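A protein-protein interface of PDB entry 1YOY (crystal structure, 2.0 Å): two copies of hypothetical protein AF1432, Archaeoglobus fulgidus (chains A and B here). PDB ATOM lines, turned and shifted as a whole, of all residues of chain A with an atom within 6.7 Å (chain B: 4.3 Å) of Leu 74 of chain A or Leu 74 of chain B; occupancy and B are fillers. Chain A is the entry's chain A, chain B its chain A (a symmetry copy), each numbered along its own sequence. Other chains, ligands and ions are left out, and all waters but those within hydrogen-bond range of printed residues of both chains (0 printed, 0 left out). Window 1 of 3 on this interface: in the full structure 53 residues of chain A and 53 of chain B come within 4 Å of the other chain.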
ATOM      1  N   LEU A  22     -25.219 -19.889 -27.945  1.00  0.00           N
ATOM      2  CA  LEU A  22     -24.447 -19.951 -26.685  1.00  0.00           C
ATOM      3  C   LEU A  22     -25.320 -20.058 -25.437  1.00  0.00           C
ATOM      4  O   LEU A  22     -24.827 -20.458 -24.403  1.00  0.00           O
ATOM      5  CB  LEU A  22     -23.465 -18.774 -26.578  1.00  0.00           C
ATOM      6  CG  LEU A  22     -22.491 -18.830 -27.763  1.00  0.00           C
ATOM      7  CD1 LEU A  22     -21.793 -17.527 -27.878  1.00  0.00           C
ATOM      8  CD2 LEU A  22     -21.483 -19.984 -27.564  1.00  0.00           C
ATOM      9  N   ALA A  42     -23.087 -18.609 -22.646  1.00  0.00           N
ATOM     10  CA  ALA A  42     -23.653 -17.249 -22.559  1.00  0.00           C
ATOM     11  C   ALA A  42     -23.688 -16.695 -21.136  1.00  0.00           C
ATOM     12  O   ALA A  42     -23.313 -15.527 -20.906  1.00  0.00           O
ATOM     13  CB  ALA A  42     -25.054 -17.208 -23.205  1.00  0.00           C
ATOM     14  N   SER A  45     -20.199 -15.805 -20.009  1.00  0.00           N
ATOM     15  CA  SER A  45     -19.624 -14.635 -20.713  1.00  0.00           C
ATOM     16  C   SER A  45     -20.313 -13.382 -20.138  1.00  0.00           C
ATOM     17  O   SER A  45     -19.651 -12.359 -19.945  1.00  0.00           O
ATOM     18  CB  SER A  45     -19.831 -14.683 -22.246  1.00  0.00           C
ATOM     19  OG  SER A  45     -19.238 -15.839 -22.853  1.00  0.00           O
ATOM     20  N   PHE A  46     -21.628 -13.492 -19.871  1.00  0.00           N
ATOM     21  CA  PHE A  46     -22.379 -12.459 -19.102  1.00  0.00           C
ATOM     22  C   PHE A  46     -21.632 -11.988 -17.853  1.00  0.00           C
ATOM     23  O   PHE A  46     -21.319 -10.798 -17.688  1.00  0.00           O
ATOM     24  CB  PHE A  46     -23.822 -12.965 -18.736  1.00  0.00           C
ATOM     25  CG  PHE A  46     -24.554 -12.086 -17.758  1.00  0.00           C
ATOM     26  CD1 PHE A  46     -25.117 -10.868 -18.153  1.00  0.00           C
ATOM     27  CD2 PHE A  46     -24.738 -12.495 -16.433  1.00  0.00           C
ATOM     28  CE1 PHE A  46     -25.764 -10.043 -17.209  1.00  0.00           C
ATOM     29  CE2 PHE A  46     -25.403 -11.667 -15.523  1.00  0.00           C
ATOM     30  CZ  PHE A  46     -25.901 -10.451 -15.913  1.00  0.00           C
ATOM     31  N   ARG A  47     -21.362 -12.918 -16.936  1.00  0.00           N
ATOM     32  CA  ARG A  47     -20.741 -12.502 -15.700  1.00  0.00           C
ATOM     33  C   ARG A  47     -19.260 -12.182 -15.833  1.00  0.00           C
ATOM     34  O   ARG A  47     -18.775 -11.286 -15.120  1.00  0.00           O
ATOM     35  CB  ARG A  47     -20.924 -13.513 -14.593  1.00  0.00           C
ATOM     36  CG  ARG A  47     -20.287 -12.996 -13.241  1.00  0.00           C
ATOM     37  CD  ARG A  47     -20.903 -13.703 -12.004  1.00  0.00           C
ATOM     38  NE  ARG A  47     -20.556 -15.132 -12.000  1.00  0.00           N
ATOM     39  CZ  ARG A  47     -20.715 -15.911 -10.931  1.00  0.00           C
ATOM     40  NH1 ARG A  47     -21.192 -15.360  -9.850  1.00  0.00           N
ATOM     41  NH2 ARG A  47     -20.441 -17.244 -10.960  1.00  0.00           N
ATOM     42  N   ALA A  48     -18.586 -12.849 -16.773  1.00  0.00           N
ATOM     43  CA  ALA A  48     -17.163 -12.563 -17.025  1.00  0.00           C
ATOM     44  C   ALA A  48     -17.042 -11.116 -17.547  1.00  0.00           C
ATOM     45  O   ALA A  48     -16.072 -10.433 -17.229  1.00  0.00           O
ATOM     46  CB  ALA A  48     -16.548 -13.576 -18.023  1.00  0.00           C
ATOM     47  N   ALA A  49     -18.038 -10.657 -18.319  1.00  0.00           N
ATOM     48  CA  ALA A  49     -18.016  -9.277 -18.896  1.00  0.00           C
ATOM     49  C   ALA A  49     -18.145  -8.223 -17.788  1.00  0.00           C
ATOM     50  O   ALA A  49     -17.425  -7.225 -17.748  1.00  0.00           O
ATOM     51  CB  ALA A  49     -19.134  -9.112 -19.919  1.00  0.00           C
ATOM     52  N   ILE A  50     -19.082  -8.453 -16.872  1.00  0.00           N
ATOM     53  CA  ILE A  50     -19.259  -7.613 -15.742  1.00  0.00           C
ATOM     54  C   ILE A  50     -17.966  -7.669 -14.843  1.00  0.00           C
ATOM     55  O   ILE A  50     -17.515  -6.622 -14.361  1.00  0.00           O
ATOM     56  CB  ILE A  50     -20.532  -8.048 -15.045  1.00  0.00           C
ATOM     57  CG1 ILE A  50     -21.750  -7.605 -15.890  1.00  0.00           C
ATOM     58  CG2 ILE A  50     -20.612  -7.491 -13.606  1.00  0.00           C
ATOM     59  CD1 ILE A  50     -22.979  -8.337 -15.532  1.00  0.00           C
ATOM     60  N   PHE A  53     -15.253  -5.533 -16.564  1.00  0.00           N
ATOM     61  CA  PHE A  53     -15.614  -4.140 -16.263  1.00  0.00           C
ATOM     62  C   PHE A  53     -15.055  -3.713 -14.876  1.00  0.00           C
ATOM     63  O   PHE A  53     -14.341  -2.720 -14.778  1.00  0.00           O
ATOM     64  CB  PHE A  53     -17.133  -3.954 -16.323  1.00  0.00           C
ATOM     65  CG  PHE A  53     -17.592  -2.558 -16.030  1.00  0.00           C
ATOM     66  CD1 PHE A  53     -17.612  -1.580 -17.036  1.00  0.00           C
ATOM     67  CD2 PHE A  53     -18.012  -2.206 -14.738  1.00  0.00           C
ATOM     68  CE1 PHE A  53     -18.069  -0.269 -16.758  1.00  0.00           C
ATOM     69  CE2 PHE A  53     -18.479  -0.880 -14.462  1.00  0.00           C
ATOM     70  CZ  PHE A  53     -18.482   0.073 -15.493  1.00  0.00           C
ATOM     71  N   ALA A  69     -13.479  -3.545 -22.128  1.00  0.00           N
ATOM     72  CA  ALA A  69     -13.143  -4.824 -21.482  1.00  0.00           C
ATOM     73  C   ALA A  69     -14.359  -5.723 -21.340  1.00  0.00           C
ATOM     74  O   ALA A  69     -14.275  -6.924 -21.611  1.00  0.00           O
ATOM     75  CB  ALA A  69     -12.511  -4.581 -20.106  1.00  0.00           C
ATOM     76  N   ALA A  70     -15.475  -5.164 -20.866  1.00  0.00           N
ATOM     77  CA  ALA A  70     -16.742  -5.901 -20.867  1.00  0.00           C
ATOM     78  C   ALA A  70     -17.090  -6.511 -22.207  1.00  0.00           C
ATOM     79  O   ALA A  70     -17.413  -7.676 -22.288  1.00  0.00           O
ATOM     80  CB  ALA A  70     -17.922  -5.026 -20.359  1.00  0.00           C
ATOM     81  N   THR A  71     -17.047  -5.699 -23.244  1.00  0.00           N
ATOM     82  CA  THR A  71     -17.474  -6.105 -24.586  1.00  0.00           C
ATOM     83  C   THR A  71     -16.558  -7.158 -25.162  1.00  0.00           C
ATOM     84  O   THR A  71     -17.019  -8.171 -25.737  1.00  0.00           O
ATOM     85  CB  THR A  71     -17.510  -4.868 -25.551  1.00  0.00           C
ATOM     86  OG1 THR A  71     -18.373  -3.871 -24.994  1.00  0.00           O
ATOM     87  CG2 THR A  71     -18.125  -5.264 -26.889  1.00  0.00           C
ATOM     88  N   ALA A  72     -15.256  -6.942 -24.988  1.00  0.00           N
ATOM     89  CA  ALA A  72     -14.263  -7.905 -25.375  1.00  0.00           C
ATOM     90  C   ALA A  72     -14.527  -9.287 -24.696  1.00  0.00           C
ATOM     91  O   ALA A  72     -14.383 -10.346 -25.333  1.00  0.00           O
ATOM     92  CB  ALA A  72     -12.834  -7.356 -25.020  1.00  0.00           C
ATOM     93  N   ALA A  73     -14.932  -9.262 -23.437  1.00  0.00           N
ATOM     94  CA  ALA A  73     -15.251 -10.501 -22.685  1.00  0.00           C
ATOM     95  C   ALA A  73     -16.508 -11.172 -23.269  1.00  0.00           C
ATOM     96  O   ALA A  73     -16.573 -12.392 -23.405  1.00  0.00           O
ATOM     97  CB  ALA A  73     -15.473 -10.184 -21.170  1.00  0.00           C
ATOM     98  N   LEU A  74     -17.466 -10.347 -23.689  1.00  0.00           N
ATOM     99  CA  LEU A  74     -18.668 -10.861 -24.342  1.00  0.00           C
ATOM    100  C   LEU A  74     -18.376 -11.575 -25.627  1.00  0.00           C
ATOM    101  O   LEU A  74     -19.026 -12.597 -25.898  1.00  0.00           O
ATOM    102  CB  LEU A  74     -19.665  -9.755 -24.667  1.00  0.00           C
ATOM    103  CG  LEU A  74     -20.421  -9.116 -23.520  1.00  0.00           C
ATOM    104  CD1 LEU A  74     -21.300  -7.986 -24.124  1.00  0.00           C
ATOM    105  CD2 LEU A  74     -21.255 -10.156 -22.819  1.00  0.00           C
ATOM    106  N   PHE A  75     -17.464 -11.003 -26.439  1.00  0.00           N
ATOM    107  CA  PHE A  75     -17.055 -11.553 -27.733  1.00  0.00           C
ATOM    108  C   PHE A  75     -16.092 -12.723 -27.647  1.00  0.00           C
ATOM    109  O   PHE A  75     -15.893 -13.441 -28.621  1.00  0.00           O
ATOM    110  CB  PHE A  75     -16.400 -10.461 -28.594  1.00  0.00           C
ATOM    111  CG  PHE A  75     -17.405  -9.609 -29.331  1.00  0.00           C
ATOM    112  CD1 PHE A  75     -18.063  -8.553 -28.695  1.00  0.00           C
ATOM    113  CD2 PHE A  75     -17.751  -9.914 -30.675  1.00  0.00           C
ATOM    114  CE1 PHE A  75     -19.041  -7.763 -29.378  1.00  0.00           C
ATOM    115  CE2 PHE A  75     -18.747  -9.152 -31.371  1.00  0.00           C
ATOM    116  CZ  PHE A  75     -19.386  -8.076 -30.703  1.00  0.00           C
ATOM    117  N   HIS A  76     -15.490 -12.908 -26.475  1.00  0.00           N
ATOM    118  CA  HIS A  76     -14.365 -13.828 -26.335  1.00  0.00           C
ATOM    119  C   HIS A  76     -14.739 -15.296 -26.591  1.00  0.00           C
ATOM    120  O   HIS A  76     -13.960 -16.044 -27.183  1.00  0.00           O
ATOM    121  CB  HIS A  76     -13.723 -13.697 -24.961  1.00  0.00           C
ATOM    122  CG  HIS A  76     -12.565 -14.623 -24.777  1.00  0.00           C
ATOM    123  ND1 HIS A  76     -12.680 -15.850 -24.156  1.00  0.00           N
ATOM    124  CD2 HIS A  76     -11.280 -14.521 -25.186  1.00  0.00           C
ATOM    125  CE1 HIS A  76     -11.507 -16.457 -24.172  1.00  0.00           C
ATOM    126  NE2 HIS A  76     -10.640 -15.668 -24.782  1.00  0.00           N
ATOM    127  N   ASP A  77     -15.934 -15.696 -26.170  1.00  0.00           N
ATOM    128  CA  ASP A  77     -16.354 -17.091 -26.323  1.00  0.00           C
ATOM    129  C   ASP A  77     -17.335 -17.344 -27.457  1.00  0.00           C
ATOM    130  O   ASP A  77     -17.859 -18.443 -27.557  1.00  0.00           O
ATOM    131  CB  ASP A  77     -17.021 -17.581 -25.041  1.00  0.00           C
ATOM    132  CG  ASP A  77     -16.069 -17.625 -23.866  1.00  0.00           C
ATOM    133  OD1 ASP A  77     -14.927 -18.152 -24.010  1.00  0.00           O
ATOM    134  OD2 ASP A  77     -16.473 -17.086 -22.814  1.00  0.00           O
ATOM    135  N   LEU A  78     -17.615 -16.339 -28.287  1.00  0.00           N
ATOM    136  CA  LEU A  78     -18.578 -16.502 -29.388  1.00  0.00           C
ATOM    137  C   LEU A  78     -18.217 -17.673 -30.330  1.00  0.00           C
ATOM    138  O   LEU A  78     -19.112 -18.394 -30.830  1.00  0.00           O
ATOM    139  CB  LEU A  78     -18.695 -15.217 -30.191  1.00  0.00           C
ATOM    140  CG  LEU A  78     -19.423 -14.070 -29.495  1.00  0.00           C
ATOM    141  CD1 LEU A  78     -19.648 -12.942 -30.457  1.00  0.00           C
ATOM    142  CD2 LEU A  78     -20.776 -14.489 -28.837  1.00  0.00           C
ATOM    143  N   VAL A 122      -9.840  -9.477 -19.809  1.00  0.00           N
ATOM    144  CA  VAL A 122     -10.741 -10.556 -20.280  1.00  0.00           C
ATOM    145  C   VAL A 122     -10.217 -11.911 -19.777  1.00  0.00           C
ATOM    146  O   VAL A 122     -10.977 -12.766 -19.269  1.00  0.00           O
ATOM    147  CB  VAL A 122     -10.799 -10.610 -21.826  1.00  0.00           C
ATOM    148  CG1 VAL A 122     -11.695 -11.787 -22.316  1.00  0.00           C
ATOM    149  CG2 VAL A 122     -11.337  -9.281 -22.416  1.00  0.00           C
ATOM    150  N   SER B  45     -29.492 -10.910 -21.267  1.00  0.00           N
ATOM    151  CA  SER B  45     -28.711  -9.657 -21.156  1.00  0.00           C
ATOM    152  C   SER B  45     -27.429  -9.852 -21.990  1.00  0.00           C
ATOM    153  O   SER B  45     -26.994  -8.914 -22.663  1.00  0.00           O
ATOM    154  CB  SER B  45     -28.331  -9.301 -19.698  1.00  0.00           C
ATOM    155  OG  SER B  45     -29.475  -9.128 -18.850  1.00  0.00           O
ATOM    156  N   PHE B  46     -26.857 -11.069 -21.932  1.00  0.00           N
ATOM    157  CA  PHE B  46     -25.760 -11.484 -22.853  1.00  0.00           C
ATOM    158  C   PHE B  46     -26.032 -11.106 -24.309  1.00  0.00           C
ATOM    159  O   PHE B  46     -25.265 -10.367 -24.946  1.00  0.00           O
ATOM    160  CB  PHE B  46     -25.461 -13.022 -22.717  1.00  0.00           C
ATOM    161  CG  PHE B  46     -24.543 -13.567 -23.777  1.00  0.00           C
ATOM    162  CD1 PHE B  46     -23.164 -13.329 -23.739  1.00  0.00           C
ATOM    163  CD2 PHE B  46     -25.040 -14.376 -24.805  1.00  0.00           C
ATOM    164  CE1 PHE B  46     -22.328 -13.816 -24.765  1.00  0.00           C
ATOM    165  CE2 PHE B  46     -24.184 -14.864 -25.797  1.00  0.00           C
ATOM    166  CZ  PHE B  46     -22.845 -14.576 -25.776  1.00  0.00           C
ATOM    167  N   ALA B  49     -26.808  -7.403 -25.075  1.00  0.00           N
ATOM    168  CA  ALA B  49     -25.579  -6.548 -25.046  1.00  0.00           C
ATOM    169  C   ALA B  49     -24.871  -6.568 -26.408  1.00  0.00           C
ATOM    170  O   ALA B  49     -24.457  -5.540 -26.943  1.00  0.00           O
ATOM    171  CB  ALA B  49     -24.633  -7.020 -23.948  1.00  0.00           C
ATOM    172  N   ILE B  50     -24.732  -7.763 -26.974  1.00  0.00           N
ATOM    173  CA  ILE B  50     -24.177  -7.928 -28.270  1.00  0.00           C
ATOM    174  C   ILE B  50     -25.105  -7.219 -29.328  1.00  0.00           C
ATOM    175  O   ILE B  50     -24.592  -6.546 -30.231  1.00  0.00           O
ATOM    176  CB  ILE B  50     -23.978  -9.412 -28.496  1.00  0.00           C
ATOM    177  CG1 ILE B  50     -22.787  -9.902 -27.640  1.00  0.00           C
ATOM    178  CG2 ILE B  50     -23.768  -9.738 -29.992  1.00  0.00           C
ATOM    179  CD1 ILE B  50     -22.786 -11.365 -27.460  1.00  0.00           C
ATOM    180  N   ALA B  70     -23.214  -1.898 -25.221  1.00  0.00           N
ATOM    181  CA  ALA B  70     -23.126  -3.267 -24.705  1.00  0.00           C
ATOM    182  C   ALA B  70     -23.167  -3.351 -23.195  1.00  0.00           C
ATOM    183  O   ALA B  70     -23.925  -4.116 -22.641  1.00  0.00           O
ATOM    184  CB  ALA B  70     -21.872  -4.011 -25.245  1.00  0.00           C
ATOM    185  N   THR B  71     -22.320  -2.576 -22.547  1.00  0.00           N
ATOM    186  CA  THR B  71     -22.152  -2.631 -21.092  1.00  0.00           C
ATOM    187  C   THR B  71     -23.394  -2.158 -20.374  1.00  0.00           C
ATOM    188  O   THR B  71     -23.854  -2.793 -19.395  1.00  0.00           O
ATOM    189  CB  THR B  71     -20.931  -1.751 -20.645  1.00  0.00           C
ATOM    190  OG1 THR B  71     -19.761  -2.199 -21.337  1.00  0.00           O
ATOM    191  CG2 THR B  71     -20.652  -1.956 -19.160  1.00  0.00           C
ATOM    192  N   ALA B  72     -23.960  -1.061 -20.869  1.00  0.00           N
ATOM    193  CA  ALA B  72     -25.208  -0.554 -20.370  1.00  0.00           C
ATOM    194  C   ALA B  72     -26.326  -1.641 -20.445  1.00  0.00           C
ATOM    195  O   ALA B  72     -27.140  -1.779 -19.515  1.00  0.00           O
ATOM    196  CB  ALA B  72     -25.608   0.735 -21.176  1.00  0.00           C
ATOM    197  N   ALA B  73     -26.337  -2.409 -21.523  1.00  0.00           N
ATOM    198  CA  ALA B  73     -27.324  -3.503 -21.703  1.00  0.00           C
ATOM    199  C   ALA B  73     -27.071  -4.625 -20.680  1.00  0.00           C
ATOM    200  O   ALA B  73     -28.003  -5.186 -20.108  1.00  0.00           O
ATOM    201  CB  ALA B  73     -27.247  -4.078 -23.155  1.00  0.00           C
ATOM    202  N   LEU B  74     -25.793  -4.880 -20.400  1.00  0.00           N
ATOM    203  CA  LEU B  74     -25.429  -5.861 -19.380  1.00  0.00           C
ATOM    204  C   LEU B  74     -25.913  -5.492 -18.011  1.00  0.00           C
ATOM    205  O   LEU B  74     -26.339  -6.391 -17.270  1.00  0.00           O
ATOM    206  CB  LEU B  74     -23.921  -6.053 -19.279  1.00  0.00           C
ATOM    207  CG  LEU B  74     -23.217  -6.787 -20.402  1.00  0.00           C
ATOM    208  CD1 LEU B  74     -21.698  -6.773 -20.078  1.00  0.00           C
ATOM    209  CD2 LEU B  74     -23.752  -8.193 -20.505  1.00  0.00           C
ATOM    210  N   PHE B  75     -25.781  -4.196 -17.656  1.00  0.00           N
ATOM    211  CA  PHE B  75     -26.193  -3.653 -16.361  1.00  0.00           C
ATOM    212  C   PHE B  75     -27.687  -3.433 -16.214  1.00  0.00           C
ATOM    213  O   PHE B  75     -28.187  -3.251 -15.108  1.00  0.00           O
ATOM    214  CB  PHE B  75     -25.487  -2.313 -16.095  1.00  0.00           C
ATOM    215  CG  PHE B  75     -24.099  -2.481 -15.525  1.00  0.00           C
ATOM    216  CD1 PHE B  75     -23.008  -2.763 -16.351  1.00  0.00           C
ATOM    217  CD2 PHE B  75     -23.891  -2.423 -14.121  1.00  0.00           C
ATOM    218  CE1 PHE B  75     -21.695  -2.956 -15.814  1.00  0.00           C
ATOM    219  CE2 PHE B  75     -22.589  -2.639 -13.559  1.00  0.00           C
ATOM    220  CZ  PHE B  75     -21.498  -2.908 -14.424  1.00  0.00           C
ATOM    221  N   HIS B  76     -28.400  -3.444 -17.338  1.00  0.00           N
ATOM    222  CA  HIS B  76     -29.789  -2.997 -17.362  1.00  0.00           C
ATOM    223  C   HIS B  76     -30.731  -3.880 -16.530  1.00  0.00           C
ATOM    224  O   HIS B  76     -31.647  -3.375 -15.879  1.00  0.00           O
ATOM    225  CB  HIS B  76     -30.306  -2.903 -18.791  1.00  0.00           C
ATOM    226  CG  HIS B  76     -31.727  -2.447 -18.860  1.00  0.00           C
ATOM    227  ND1 HIS B  76     -32.788  -3.323 -18.966  1.00  0.00           N
ATOM    228  CD2 HIS B  76     -32.261  -1.208 -18.780  1.00  0.00           C
ATOM    229  CE1 HIS B  76     -33.918  -2.637 -18.969  1.00  0.00           C
ATOM    230  NE2 HIS B  76     -33.624  -1.353 -18.868  1.00  0.00           N
ATOM    231  N   LEU B  78     -29.680  -6.096 -14.036  1.00  0.00           N
ATOM    232  CA  LEU B  78     -29.070  -6.563 -12.781  1.00  0.00           C
ATOM    233  C   LEU B  78     -30.032  -6.467 -11.576  1.00  0.00           C
ATOM    234  O   LEU B  78     -30.034  -7.348 -10.684  1.00  0.00           O
ATOM    235  CB  LEU B  78     -27.798  -5.785 -12.483  1.00  0.00           C
ATOM    236  CG  LEU B  78     -26.606  -6.103 -13.382  1.00  0.00           C
ATOM    237  CD1 LEU B  78     -25.372  -5.429 -12.861  1.00  0.00           C
ATOM    238  CD2 LEU B  78     -26.343  -7.632 -13.563  1.00  0.00           C
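CB of Ser 45 of chain A touches CE1 of Phe 46 of chain B, 3.7 Å away.
Phe 46 of chain A touches Ser 45 of chain B (CE1 to CB, 3.7 Å).
Phe 46 of chain A touches Leu 74 of chain B.
Leu 78 of chain B touches Ile 50 of chain A.
Phe 53 of chain A touches Thr 71 of chain B.
Phe 53 of chain A touches Phe 75 of chain B.
CB of Ala 70 of chain B touches OG1 of Thr 71 of chain A (3.5 Å).
Phe 46 of chain B touches Leu 74 of chain A (CE1 to O, 3.7 Å).
Leu 74 of chain A touches Ala 49 of chain B.
Ile 50 of chain B touches Leu 78 of chain A.
O of Leu 22 of chain A sits at hydrogen-bond distance from N of Ala 42 of chain A.
OG of Ser 45 of chain A sits at hydrogen-bond distance from OD2 of Asp 77 of chain A (3.0 Å).
Printed residues of chain B that touch a printed residue of chain A: Ser 45, Phe 46, Ala 49, Ile 50, Ala 70, Thr 71, Leu 74, Phe 75 and Leu 78.
Hydrophobic or aromatic side chains of chain B that line the printed part of chain A: Phe 46, Ala 49, Ile 50, Ala 70, Leu 74, Phe 75 and Leu 78.
Among the printed residues, 17 pairs touch across the chains.
Among the printed residues, no Asp or Glu carboxylate lies within 4 Å of a Lys or Arg side-chain nitrogen of the other chain.
Ser 45 of chain A touches Phe 46 of chain B, and with the chains exchanged Phe 46 of chain A touches Ser 45 of chain B.
Phe 46 of chain A touches Leu 74 of chain B, and with the chains exchanged Leu 74 of chain A touches Phe 46 of chain B.
Phe 46 of chain A touches Leu 78 of chain B, and with the chains exchanged Leu 78 of chain A touches Phe 46 of chain B.
Ala 49 of chain A touches Leu 74 of chain B, and with the chains exchanged Leu 74 of chain A touches Ala 49 of chain B.
12 positions are printed for both chains.
Of the 17 pairs that touch across the chains among the printed residues, 13 have their exchanged pair printed and touching as well.
Of chain B, only Phe 46, Ala 49 and Leu 74 come within 4 Å of Leu 74 of chain A.
Of chain A, only Phe 46, Ala 49 and Leu 74 come within 4 Å of Leu 74 of chain B.
Printed residues of chain A within 4 Å of Ser 45 of chain B: Phe 46.
Printed residues of chain B within 4 Å of Leu 78 of chain A: Phe 46 (3.7 Å) and Ile 50 (3.96 Å).
Of the printed residues of chain A, Ala 49 of chain B touches Leu 74.
Printed residues of chain B within 4 Å of Ala 70 of chain A: Thr 71.
Ala 69 of chain A touches none of the printed residues of chain B.
His 76 of chain B touches none of the printed residues of chain A.
The nearest printed residue of chain B that does not touch Thr 71 of chain A is Thr 71 of chain B (4.3 Å).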
